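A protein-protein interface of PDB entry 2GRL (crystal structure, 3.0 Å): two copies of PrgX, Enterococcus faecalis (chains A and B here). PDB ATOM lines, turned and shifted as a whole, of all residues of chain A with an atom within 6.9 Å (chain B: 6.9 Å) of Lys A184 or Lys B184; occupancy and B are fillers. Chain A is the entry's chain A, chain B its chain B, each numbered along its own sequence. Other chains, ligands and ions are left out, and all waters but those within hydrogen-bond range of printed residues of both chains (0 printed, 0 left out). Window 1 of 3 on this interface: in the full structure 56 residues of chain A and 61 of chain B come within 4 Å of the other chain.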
ATOM      1  N   ASN A  63     -28.779 -25.720  15.531  1.00  0.00           N
ATOM      2  CA  ASN A  63     -28.217 -24.652  14.718  1.00  0.00           C
ATOM      3  C   ASN A  63     -29.256 -24.154  13.698  1.00  0.00           C
ATOM      4  O   ASN A  63     -29.488 -22.949  13.546  1.00  0.00           O
ATOM      5  CB  ASN A  63     -26.979 -25.154  13.988  1.00  0.00           C
ATOM      6  CG  ASN A  63     -26.256 -24.050  13.250  1.00  0.00           C
ATOM      7  OD1 ASN A  63     -26.751 -23.523  12.251  1.00  0.00           O
ATOM      8  ND2 ASN A  63     -25.078 -23.684  13.746  1.00  0.00           N
ATOM      9  N   SER A 181     -12.417 -33.566  26.515  1.00  0.00           N
ATOM     10  CA  SER A 181     -12.890 -32.663  25.479  1.00  0.00           C
ATOM     11  C   SER A 181     -14.355 -32.380  25.743  1.00  0.00           C
ATOM     12  O   SER A 181     -15.119 -33.281  26.062  1.00  0.00           O
ATOM     13  CB  SER A 181     -12.734 -33.296  24.100  1.00  0.00           C
ATOM     14  OG  SER A 181     -13.423 -32.530  23.131  1.00  0.00           O
ATOM     15  N   PHE A 182     -14.748 -31.125  25.626  1.00  0.00           N
ATOM     16  CA  PHE A 182     -16.136 -30.786  25.847  1.00  0.00           C
ATOM     17  C   PHE A 182     -16.715 -30.022  24.664  1.00  0.00           C
ATOM     18  O   PHE A 182     -17.412 -29.017  24.828  1.00  0.00           O
ATOM     19  CB  PHE A 182     -16.284 -29.988  27.140  1.00  0.00           C
ATOM     20  CG  PHE A 182     -15.956 -30.778  28.367  1.00  0.00           C
ATOM     21  CD1 PHE A 182     -16.773 -31.842  28.770  1.00  0.00           C
ATOM     22  CD2 PHE A 182     -14.812 -30.492  29.104  1.00  0.00           C
ATOM     23  CE1 PHE A 182     -16.446 -32.609  29.889  1.00  0.00           C
ATOM     24  CE2 PHE A 182     -14.475 -31.253  30.227  1.00  0.00           C
ATOM     25  CZ  PHE A 182     -15.291 -32.312  30.618  1.00  0.00           C
ATOM     26  N   GLY A 183     -16.411 -30.515  23.466  1.00  0.00           N
ATOM     27  CA  GLY A 183     -16.931 -29.897  22.260  1.00  0.00           C
ATOM     28  C   GLY A 183     -15.925 -29.078  21.482  1.00  0.00           C
ATOM     29  O   GLY A 183     -14.904 -28.640  22.031  1.00  0.00           O
ATOM     30  N   LYS A 184     -16.238 -28.862  20.205  1.00  0.00           N
ATOM     31  CA  LYS A 184     -15.382 -28.109  19.298  1.00  0.00           C
ATOM     32  C   LYS A 184     -14.998 -26.744  19.886  1.00  0.00           C
ATOM     33  O   LYS A 184     -13.815 -26.385  19.939  1.00  0.00           O
ATOM     34  CB  LYS A 184     -16.084 -27.918  17.947  1.00  0.00           C
ATOM     35  CG  LYS A 184     -16.765 -29.178  17.402  1.00  0.00           C
ATOM     36  CD  LYS A 184     -15.798 -30.349  17.275  1.00  0.00           C
ATOM     37  CE  LYS A 184     -16.492 -31.602  16.748  1.00  0.00           C
ATOM     38  NZ  LYS A 184     -16.952 -31.444  15.340  1.00  0.00           N
ATOM     39  N   ASP A 185     -15.998 -25.993  20.338  1.00  0.00           N
ATOM     40  CA  ASP A 185     -15.772 -24.674  20.910  1.00  0.00           C
ATOM     41  C   ASP A 185     -14.797 -24.713  22.086  1.00  0.00           C
ATOM     42  O   ASP A 185     -13.926 -23.843  22.221  1.00  0.00           O
ATOM     43  CB  ASP A 185     -17.105 -24.078  21.347  1.00  0.00           C
ATOM     44  CG  ASP A 185     -18.003 -23.742  20.173  1.00  0.00           C
ATOM     45  OD1 ASP A 185     -19.244 -23.824  20.324  1.00  0.00           O
ATOM     46  OD2 ASP A 185     -17.461 -23.387  19.100  1.00  0.00           O
ATOM     47  N   TYR A 186     -14.944 -25.721  22.940  1.00  0.00           N
ATOM     48  CA  TYR A 186     -14.069 -25.887  24.109  1.00  0.00           C
ATOM     49  C   TYR A 186     -12.645 -26.223  23.657  1.00  0.00           C
ATOM     50  O   TYR A 186     -11.677 -25.588  24.064  1.00  0.00           O
ATOM     51  CB  TYR A 186     -14.642 -27.002  25.000  1.00  0.00           C
ATOM     52  CG  TYR A 186     -13.780 -27.417  26.169  1.00  0.00           C
ATOM     53  CD1 TYR A 186     -12.823 -28.434  26.034  1.00  0.00           C
ATOM     54  CD2 TYR A 186     -13.935 -26.816  27.415  1.00  0.00           C
ATOM     55  CE1 TYR A 186     -12.052 -28.842  27.117  1.00  0.00           C
ATOM     56  CE2 TYR A 186     -13.170 -27.214  28.502  1.00  0.00           C
ATOM     57  CZ  TYR A 186     -12.235 -28.228  28.350  1.00  0.00           C
ATOM     58  OH  TYR A 186     -11.521 -28.653  29.452  1.00  0.00           O
ATOM     59  N   ASP A 187     -12.533 -27.223  22.796  1.00  0.00           N
ATOM     60  CA  ASP A 187     -11.243 -27.632  22.268  1.00  0.00           C
ATOM     61  C   ASP A 187     -10.542 -26.414  21.663  1.00  0.00           C
ATOM     62  O   ASP A 187      -9.341 -26.207  21.840  1.00  0.00           O
ATOM     63  CB  ASP A 187     -11.424 -28.703  21.168  1.00  0.00           C
ATOM     64  CG  ASP A 187     -12.094 -29.975  21.675  1.00  0.00           C
ATOM     65  OD1 ASP A 187     -12.399 -30.855  20.857  1.00  0.00           O
ATOM     66  OD2 ASP A 187     -12.319 -30.113  22.890  1.00  0.00           O
ATOM     67  N   LEU A 188     -11.312 -25.603  20.947  1.00  0.00           N
ATOM     68  CA  LEU A 188     -10.764 -24.439  20.275  1.00  0.00           C
ATOM     69  C   LEU A 188     -10.113 -23.432  21.218  1.00  0.00           C
ATOM     70  O   LEU A 188      -8.951 -23.068  21.032  1.00  0.00           O
ATOM     71  CB  LEU A 188     -11.860 -23.781  19.424  1.00  0.00           C
ATOM     72  CG  LEU A 188     -11.464 -22.813  18.297  1.00  0.00           C
ATOM     73  CD1 LEU A 188     -11.180 -21.454  18.872  1.00  0.00           C
ATOM     74  CD2 LEU A 188     -10.248 -23.337  17.550  1.00  0.00           C
ATOM     75  N   THR A 189     -10.840 -22.992  22.237  1.00  0.00           N
ATOM     76  CA  THR A 189     -10.280 -22.023  23.169  1.00  0.00           C
ATOM     77  C   THR A 189      -9.106 -22.551  23.969  1.00  0.00           C
ATOM     78  O   THR A 189      -8.169 -21.793  24.238  1.00  0.00           O
ATOM     79  CB  THR A 189     -11.314 -21.510  24.160  1.00  0.00           C
ATOM     80  OG1 THR A 189     -11.919 -22.621  24.815  1.00  0.00           O
ATOM     81  CG2 THR A 189     -12.372 -20.713  23.456  1.00  0.00           C
ATOM     82  N   GLN A 191      -6.873 -24.505  22.944  1.00  0.00           N
ATOM     83  CA  GLN A 191      -5.732 -24.469  22.036  1.00  0.00           C
ATOM     84  C   GLN A 191      -5.262 -23.041  21.846  1.00  0.00           C
ATOM     85  O   GLN A 191      -4.065 -22.766  21.831  1.00  0.00           O
ATOM     86  CB  GLN A 191      -6.096 -25.061  20.675  1.00  0.00           C
ATOM     87  CG  GLN A 191      -6.230 -26.561  20.669  1.00  0.00           C
ATOM     88  CD  GLN A 191      -6.667 -27.091  19.324  1.00  0.00           C
ATOM     89  OE1 GLN A 191      -5.954 -26.958  18.335  1.00  0.00           O
ATOM     90  NE2 GLN A 191      -7.848 -27.694  19.279  1.00  0.00           N
ATOM     91  N   ASN A 225     -11.515 -37.844  21.332  1.00  0.00           N
ATOM     92  CA  ASN A 225     -12.490 -36.911  20.786  1.00  0.00           C
ATOM     93  C   ASN A 225     -12.059 -35.449  20.745  1.00  0.00           C
ATOM     94  O   ASN A 225     -12.899 -34.567  20.576  1.00  0.00           O
ATOM     95  CB  ASN A 225     -13.813 -37.026  21.551  1.00  0.00           C
ATOM     96  CG  ASN A 225     -14.466 -38.394  21.401  1.00  0.00           C
ATOM     97  OD1 ASN A 225     -14.678 -38.880  20.287  1.00  0.00           O
ATOM     98  ND2 ASN A 225     -14.801 -39.015  22.526  1.00  0.00           N
ATOM     99  N   ILE A 226     -10.765 -35.185  20.897  1.00  0.00           N
ATOM    100  CA  ILE A 226     -10.277 -33.810  20.851  1.00  0.00           C
ATOM    101  C   ILE A 226     -10.175 -33.397  19.381  1.00  0.00           C
ATOM    102  O   ILE A 226      -9.765 -34.185  18.537  1.00  0.00           O
ATOM    103  CB  ILE A 226      -8.873 -33.683  21.506  1.00  0.00           C
ATOM    104  CG1 ILE A 226      -8.558 -32.206  21.774  1.00  0.00           C
ATOM    105  CG2 ILE A 226      -7.784 -34.310  20.594  1.00  0.00           C
ATOM    106  CD1 ILE A 226      -9.375 -31.628  22.869  1.00  0.00           C
ATOM    107  N   SER A 227     -10.560 -32.169  19.065  1.00  0.00           N
ATOM    108  CA  SER A 227     -10.466 -31.693  17.690  1.00  0.00           C
ATOM    109  C   SER A 227      -9.337 -30.689  17.584  1.00  0.00           C
ATOM    110  O   SER A 227      -9.534 -29.510  17.837  1.00  0.00           O
ATOM    111  CB  SER A 227     -11.756 -31.015  17.254  1.00  0.00           C
ATOM    112  OG  SER A 227     -12.827 -31.927  17.273  1.00  0.00           O
ATOM    113  N   ASN B  63     -22.674 -31.099  26.039  1.00  0.00           N
ATOM    114  CA  ASN B  63     -21.584 -32.051  25.897  1.00  0.00           C
ATOM    115  C   ASN B  63     -21.230 -32.626  27.261  1.00  0.00           C
ATOM    116  O   ASN B  63     -21.102 -33.829  27.428  1.00  0.00           O
ATOM    117  CB  ASN B  63     -20.364 -31.369  25.274  1.00  0.00           C
ATOM    118  CG  ASN B  63     -19.244 -32.340  24.975  1.00  0.00           C
ATOM    119  OD1 ASN B  63     -18.612 -32.881  25.882  1.00  0.00           O
ATOM    120  ND2 ASN B  63     -18.997 -32.573  23.693  1.00  0.00           N
ATOM    121  N   SER B 181     -24.024 -21.743   7.028  1.00  0.00           N
ATOM    122  CA  SER B 181     -23.306 -22.640   7.907  1.00  0.00           C
ATOM    123  C   SER B 181     -24.275 -23.100   8.976  1.00  0.00           C
ATOM    124  O   SER B 181     -25.044 -22.312   9.517  1.00  0.00           O
ATOM    125  CB  SER B 181     -22.134 -21.921   8.563  1.00  0.00           C
ATOM    126  OG  SER B 181     -21.601 -22.713   9.607  1.00  0.00           O
ATOM    127  N   PHE B 182     -24.254 -24.385   9.280  1.00  0.00           N
ATOM    128  CA  PHE B 182     -25.154 -24.906  10.293  1.00  0.00           C
ATOM    129  C   PHE B 182     -24.394 -25.698  11.338  1.00  0.00           C
ATOM    130  O   PHE B 182     -24.809 -26.787  11.746  1.00  0.00           O
ATOM    131  CB  PHE B 182     -26.246 -25.768   9.658  1.00  0.00           C
ATOM    132  CG  PHE B 182     -27.184 -24.991   8.765  1.00  0.00           C
ATOM    133  CD1 PHE B 182     -28.051 -24.032   9.313  1.00  0.00           C
ATOM    134  CD2 PHE B 182     -27.188 -25.195   7.377  1.00  0.00           C
ATOM    135  CE1 PHE B 182     -28.898 -23.299   8.498  1.00  0.00           C
ATOM    136  CE2 PHE B 182     -28.027 -24.465   6.564  1.00  0.00           C
ATOM    137  CZ  PHE B 182     -28.881 -23.517   7.122  1.00  0.00           C
ATOM    138  N   GLY B 183     -23.266 -25.143  11.764  1.00  0.00           N
ATOM    139  CA  GLY B 183     -22.496 -25.798  12.799  1.00  0.00           C
ATOM    140  C   GLY B 183     -21.230 -26.446  12.317  1.00  0.00           C
ATOM    141  O   GLY B 183     -21.121 -26.771  11.136  1.00  0.00           O
ATOM    142  N   LYS B 184     -20.292 -26.638  13.247  1.00  0.00           N
ATOM    143  CA  LYS B 184     -18.994 -27.225  12.952  1.00  0.00           C
ATOM    144  C   LYS B 184     -19.132 -28.548  12.194  1.00  0.00           C
ATOM    145  O   LYS B 184     -18.497 -28.754  11.152  1.00  0.00           O
ATOM    146  CB  LYS B 184     -18.212 -27.444  14.253  1.00  0.00           C
ATOM    147  CG  LYS B 184     -18.233 -26.259  15.221  1.00  0.00           C
ATOM    148  CD  LYS B 184     -17.718 -24.978  14.571  1.00  0.00           C
ATOM    149  CE  LYS B 184     -17.756 -23.798  15.538  1.00  0.00           C
ATOM    150  NZ  LYS B 184     -16.794 -23.957  16.661  1.00  0.00           N
ATOM    151  N   ASP B 185     -19.966 -29.439  12.716  1.00  0.00           N
ATOM    152  CA  ASP B 185     -20.189 -30.745  12.104  1.00  0.00           C
ATOM    153  C   ASP B 185     -20.672 -30.643  10.657  1.00  0.00           C
ATOM    154  O   ASP B 185     -20.240 -31.419   9.794  1.00  0.00           O
ATOM    155  CB  ASP B 185     -21.205 -31.532  12.927  1.00  0.00           C
ATOM    156  CG  ASP B 185     -20.665 -31.931  14.278  1.00  0.00           C
ATOM    157  OD1 ASP B 185     -21.460 -32.013  15.245  1.00  0.00           O
ATOM    158  OD2 ASP B 185     -19.442 -32.170  14.366  1.00  0.00           O
ATOM    159  N   TYR B 186     -21.580 -29.700  10.399  1.00  0.00           N
ATOM    160  CA  TYR B 186     -22.119 -29.474   9.058  1.00  0.00           C
ATOM    161  C   TYR B 186     -20.998 -28.958   8.141  1.00  0.00           C
ATOM    162  O   TYR B 186     -20.765 -29.510   7.056  1.00  0.00           O
ATOM    163  CB  TYR B 186     -23.272 -28.459   9.150  1.00  0.00           C
ATOM    164  CG  TYR B 186     -23.843 -27.962   7.836  1.00  0.00           C
ATOM    165  CD1 TYR B 186     -23.319 -26.828   7.193  1.00  0.00           C
ATOM    166  CD2 TYR B 186     -24.922 -28.616   7.240  1.00  0.00           C
ATOM    167  CE1 TYR B 186     -23.867 -26.362   5.992  1.00  0.00           C
ATOM    168  CE2 TYR B 186     -25.474 -28.160   6.035  1.00  0.00           C
ATOM    169  CZ  TYR B 186     -24.948 -27.039   5.422  1.00  0.00           C
ATOM    170  OH  TYR B 186     -25.517 -26.600   4.254  1.00  0.00           O
ATOM    171  N   ASP B 187     -20.306 -27.906   8.597  1.00  0.00           N
ATOM    172  CA  ASP B 187     -19.214 -27.301   7.852  1.00  0.00           C
ATOM    173  C   ASP B 187     -18.210 -28.383   7.475  1.00  0.00           C
ATOM    174  O   ASP B 187     -17.696 -28.437   6.353  1.00  0.00           O
ATOM    175  CB  ASP B 187     -18.511 -26.245   8.709  1.00  0.00           C
ATOM    176  CG  ASP B 187     -19.419 -25.097   9.106  1.00  0.00           C
ATOM    177  OD1 ASP B 187     -18.949 -24.213   9.862  1.00  0.00           O
ATOM    178  OD2 ASP B 187     -20.595 -25.070   8.668  1.00  0.00           O
ATOM    179  N   LEU B 188     -17.944 -29.258   8.431  1.00  0.00           N
ATOM    180  CA  LEU B 188     -16.981 -30.320   8.232  1.00  0.00           C
ATOM    181  C   LEU B 188     -17.329 -31.275   7.094  1.00  0.00           C
ATOM    182  O   LEU B 188     -16.517 -31.490   6.191  1.00  0.00           O
ATOM    183  CB  LEU B 188     -16.792 -31.078   9.549  1.00  0.00           C
ATOM    184  CG  LEU B 188     -15.541 -31.941   9.759  1.00  0.00           C
ATOM    185  CD1 LEU B 188     -15.742 -33.276   9.110  1.00  0.00           C
ATOM    186  CD2 LEU B 188     -14.306 -31.243   9.204  1.00  0.00           C
ATOM    187  N   THR B 189     -18.529 -31.841   7.119  1.00  0.00           N
ATOM    188  CA  THR B 189     -18.910 -32.774   6.067  1.00  0.00           C
ATOM    189  C   THR B 189     -19.016 -32.136   4.687  1.00  0.00           C
ATOM    190  O   THR B 189     -18.690 -32.787   3.680  1.00  0.00           O
ATOM    191  CB  THR B 189     -20.240 -33.469   6.366  1.00  0.00           C
ATOM    192  OG1 THR B 189     -21.239 -32.480   6.604  1.00  0.00           O
ATOM    193  CG2 THR B 189     -20.119 -34.357   7.572  1.00  0.00           C
ATOM    194  N   GLN B 191     -17.173 -29.862   3.552  1.00  0.00           N
ATOM    195  CA  GLN B 191     -15.795 -29.725   3.069  1.00  0.00           C
ATOM    196  C   GLN B 191     -15.227 -31.081   2.653  1.00  0.00           C
ATOM    197  O   GLN B 191     -14.534 -31.203   1.639  1.00  0.00           O
ATOM    198  CB  GLN B 191     -14.899 -29.122   4.145  1.00  0.00           C
ATOM    199  CG  GLN B 191     -15.110 -27.642   4.364  1.00  0.00           C
ATOM    200  CD  GLN B 191     -14.281 -27.113   5.521  1.00  0.00           C
ATOM    201  OE1 GLN B 191     -13.060 -27.097   5.460  1.00  0.00           O
ATOM    202  NE2 GLN B 191     -14.947 -26.689   6.587  1.00  0.00           N
ATOM    203  N   ASN B 225     -19.584 -17.155   9.414  1.00  0.00           N
ATOM    204  CA  ASN B 225     -19.545 -18.181  10.448  1.00  0.00           C
ATOM    205  C   ASN B 225     -19.145 -19.574   9.975  1.00  0.00           C
ATOM    206  O   ASN B 225     -19.380 -20.554  10.677  1.00  0.00           O
ATOM    207  CB  ASN B 225     -20.901 -18.268  11.159  1.00  0.00           C
ATOM    208  CG  ASN B 225     -21.260 -16.988  11.898  1.00  0.00           C
ATOM    209  OD1 ASN B 225     -20.489 -16.494  12.727  1.00  0.00           O
ATOM    210  ND2 ASN B 225     -22.443 -16.449  11.609  1.00  0.00           N
ATOM    211  N   ILE B 226     -18.546 -19.678   8.795  1.00  0.00           N
ATOM    212  CA  ILE B 226     -18.130 -20.982   8.295  1.00  0.00           C
ATOM    213  C   ILE B 226     -16.802 -21.326   8.957  1.00  0.00           C
ATOM    214  O   ILE B 226     -15.948 -20.460   9.118  1.00  0.00           O
ATOM    215  CB  ILE B 226     -17.927 -20.965   6.759  1.00  0.00           C
ATOM    216  CG1 ILE B 226     -17.850 -22.399   6.228  1.00  0.00           C
ATOM    217  CG2 ILE B 226     -16.634 -20.220   6.393  1.00  0.00           C
ATOM    218  CD1 ILE B 226     -19.166 -23.116   6.244  1.00  0.00           C
ATOM    219  N   SER B 227     -16.622 -22.578   9.352  1.00  0.00           N
ATOM    220  CA  SER B 227     -15.365 -22.982   9.976  1.00  0.00           C
ATOM    221  C   SER B 227     -14.582 -23.827   9.006  1.00  0.00           C
ATOM    222  O   SER B 227     -14.805 -25.027   8.917  1.00  0.00           O
ATOM    223  CB  SER B 227     -15.617 -23.800  11.234  1.00  0.00           C
ATOM    224  OG  SER B 227     -16.283 -23.025  12.204  1.00  0.00           O
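Of the printed residues of chain B, Ser A181 touches Asn B63 (3.5 Å).
Printed residues of chain B within 4 Å of Phe A182: Asn B63 (3.2 Å).
Of the printed residues of chain B, Lys A184 touches Lys B184 (3.8 Å) and Asp B185 (2.8 Å).
Of the printed residues of chain B, Asp A185 touches Lys B184.
Printed residues of chain A within 4 Å of Ser B181: Asn A63.
Of the printed residues of chain A, Gly B183 touches Asn A63.
Lys B184 touches two residues of chain A.
Asp B187 touches none of the printed residues of chain A.
The nearest printed residue of chain B that does not touch Lys A184 is Leu B188 (5.8 Å).
The nearest printed residue of chain A that does not touch Lys B184 is Asn A63 (5.6 Å).
Asn A63 touches Ser B181, and with the chains exchanged Ser A181 touches Asn B63.
Asn A63 touches Phe B182, and with the chains exchanged Phe A182 touches Asn B63.
Asn A63 touches Gly B183, and with the chains exchanged Gly A183 touches Asn B63.
Lys A184 touches Asp B185, and with the chains exchanged Asp A185 touches Lys B184.
Of the 9 pairs that touch across the chains among the printed residues, 9 have their exchanged pair printed and touching as well.
The side-chain carboxylate (OD2) of Asp A187 sits at hydrogen-bond distance from the side-chain hydroxyl (OG) of Ser A181, at 2.7 Å.
The backbone carbonyl oxygen (O) of Asn A225 is in hydrogen-bond range of the side-chain hydroxyl (OG) of Ser A181 (3.3 Å).
The side-chain carboxylate (OD2) of Asp B187 is in hydrogen-bond range of the side-chain hydroxyl (OG) of Ser B181 (2.7 Å).
The side-chain hydroxyl (OG) of Ser B181 is in hydrogen-bond range of the backbone carbonyl oxygen (O) of Asn B225, 3.3 Å away.
Phe B182 touches Asn A63 (CA to OD1, 2.9 Å).
Asn B63 touches Ser A181 (OD1 to O, 3.5 Å).
Asn B63 touches Phe A182.
CB of Lys A184 touches CG of Lys B184 (3.8 Å).
Of the 14 printed residues of chain A, 6 touch a printed residue of chain B.
Printed residues of chain A that touch a printed residue of chain B: Asn A63, Ser A181, Phe A182, Gly A183, Lys A184 and Asp A185.
Hydrophobic or aromatic side chains of chain A that line the printed part of chain B: Phe A182.
Among the printed residues, Asp or Glu carboxylates within 4 Å of a Lys or Arg side-chain nitrogen of the other chain: Lys A184 with Asp B185 (2.8 Å) and Asp A185 with Lys B184 (2.6 Å).
The side-chain amide oxygen (OD1) of Asn A63 lies close to the backbone carbonyl oxygen (O) of Ser B181.
The side-chain amide nitrogen (ND2) of Asn A63 sits close to the backbone NH (N) of Gly B183, 3.1 Å away.
The side-chain amide nitrogen (ND2) of Asn B63 sits close to the backbone NH (N) of Gly A183 (3.3 Å).
NZ of Lys A184 lies within salt-bridge range of OD2 of Asp B185.
OD2 of Asp A185 is in salt-bridge range of NZ of Lys B184 (2.6 Å).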
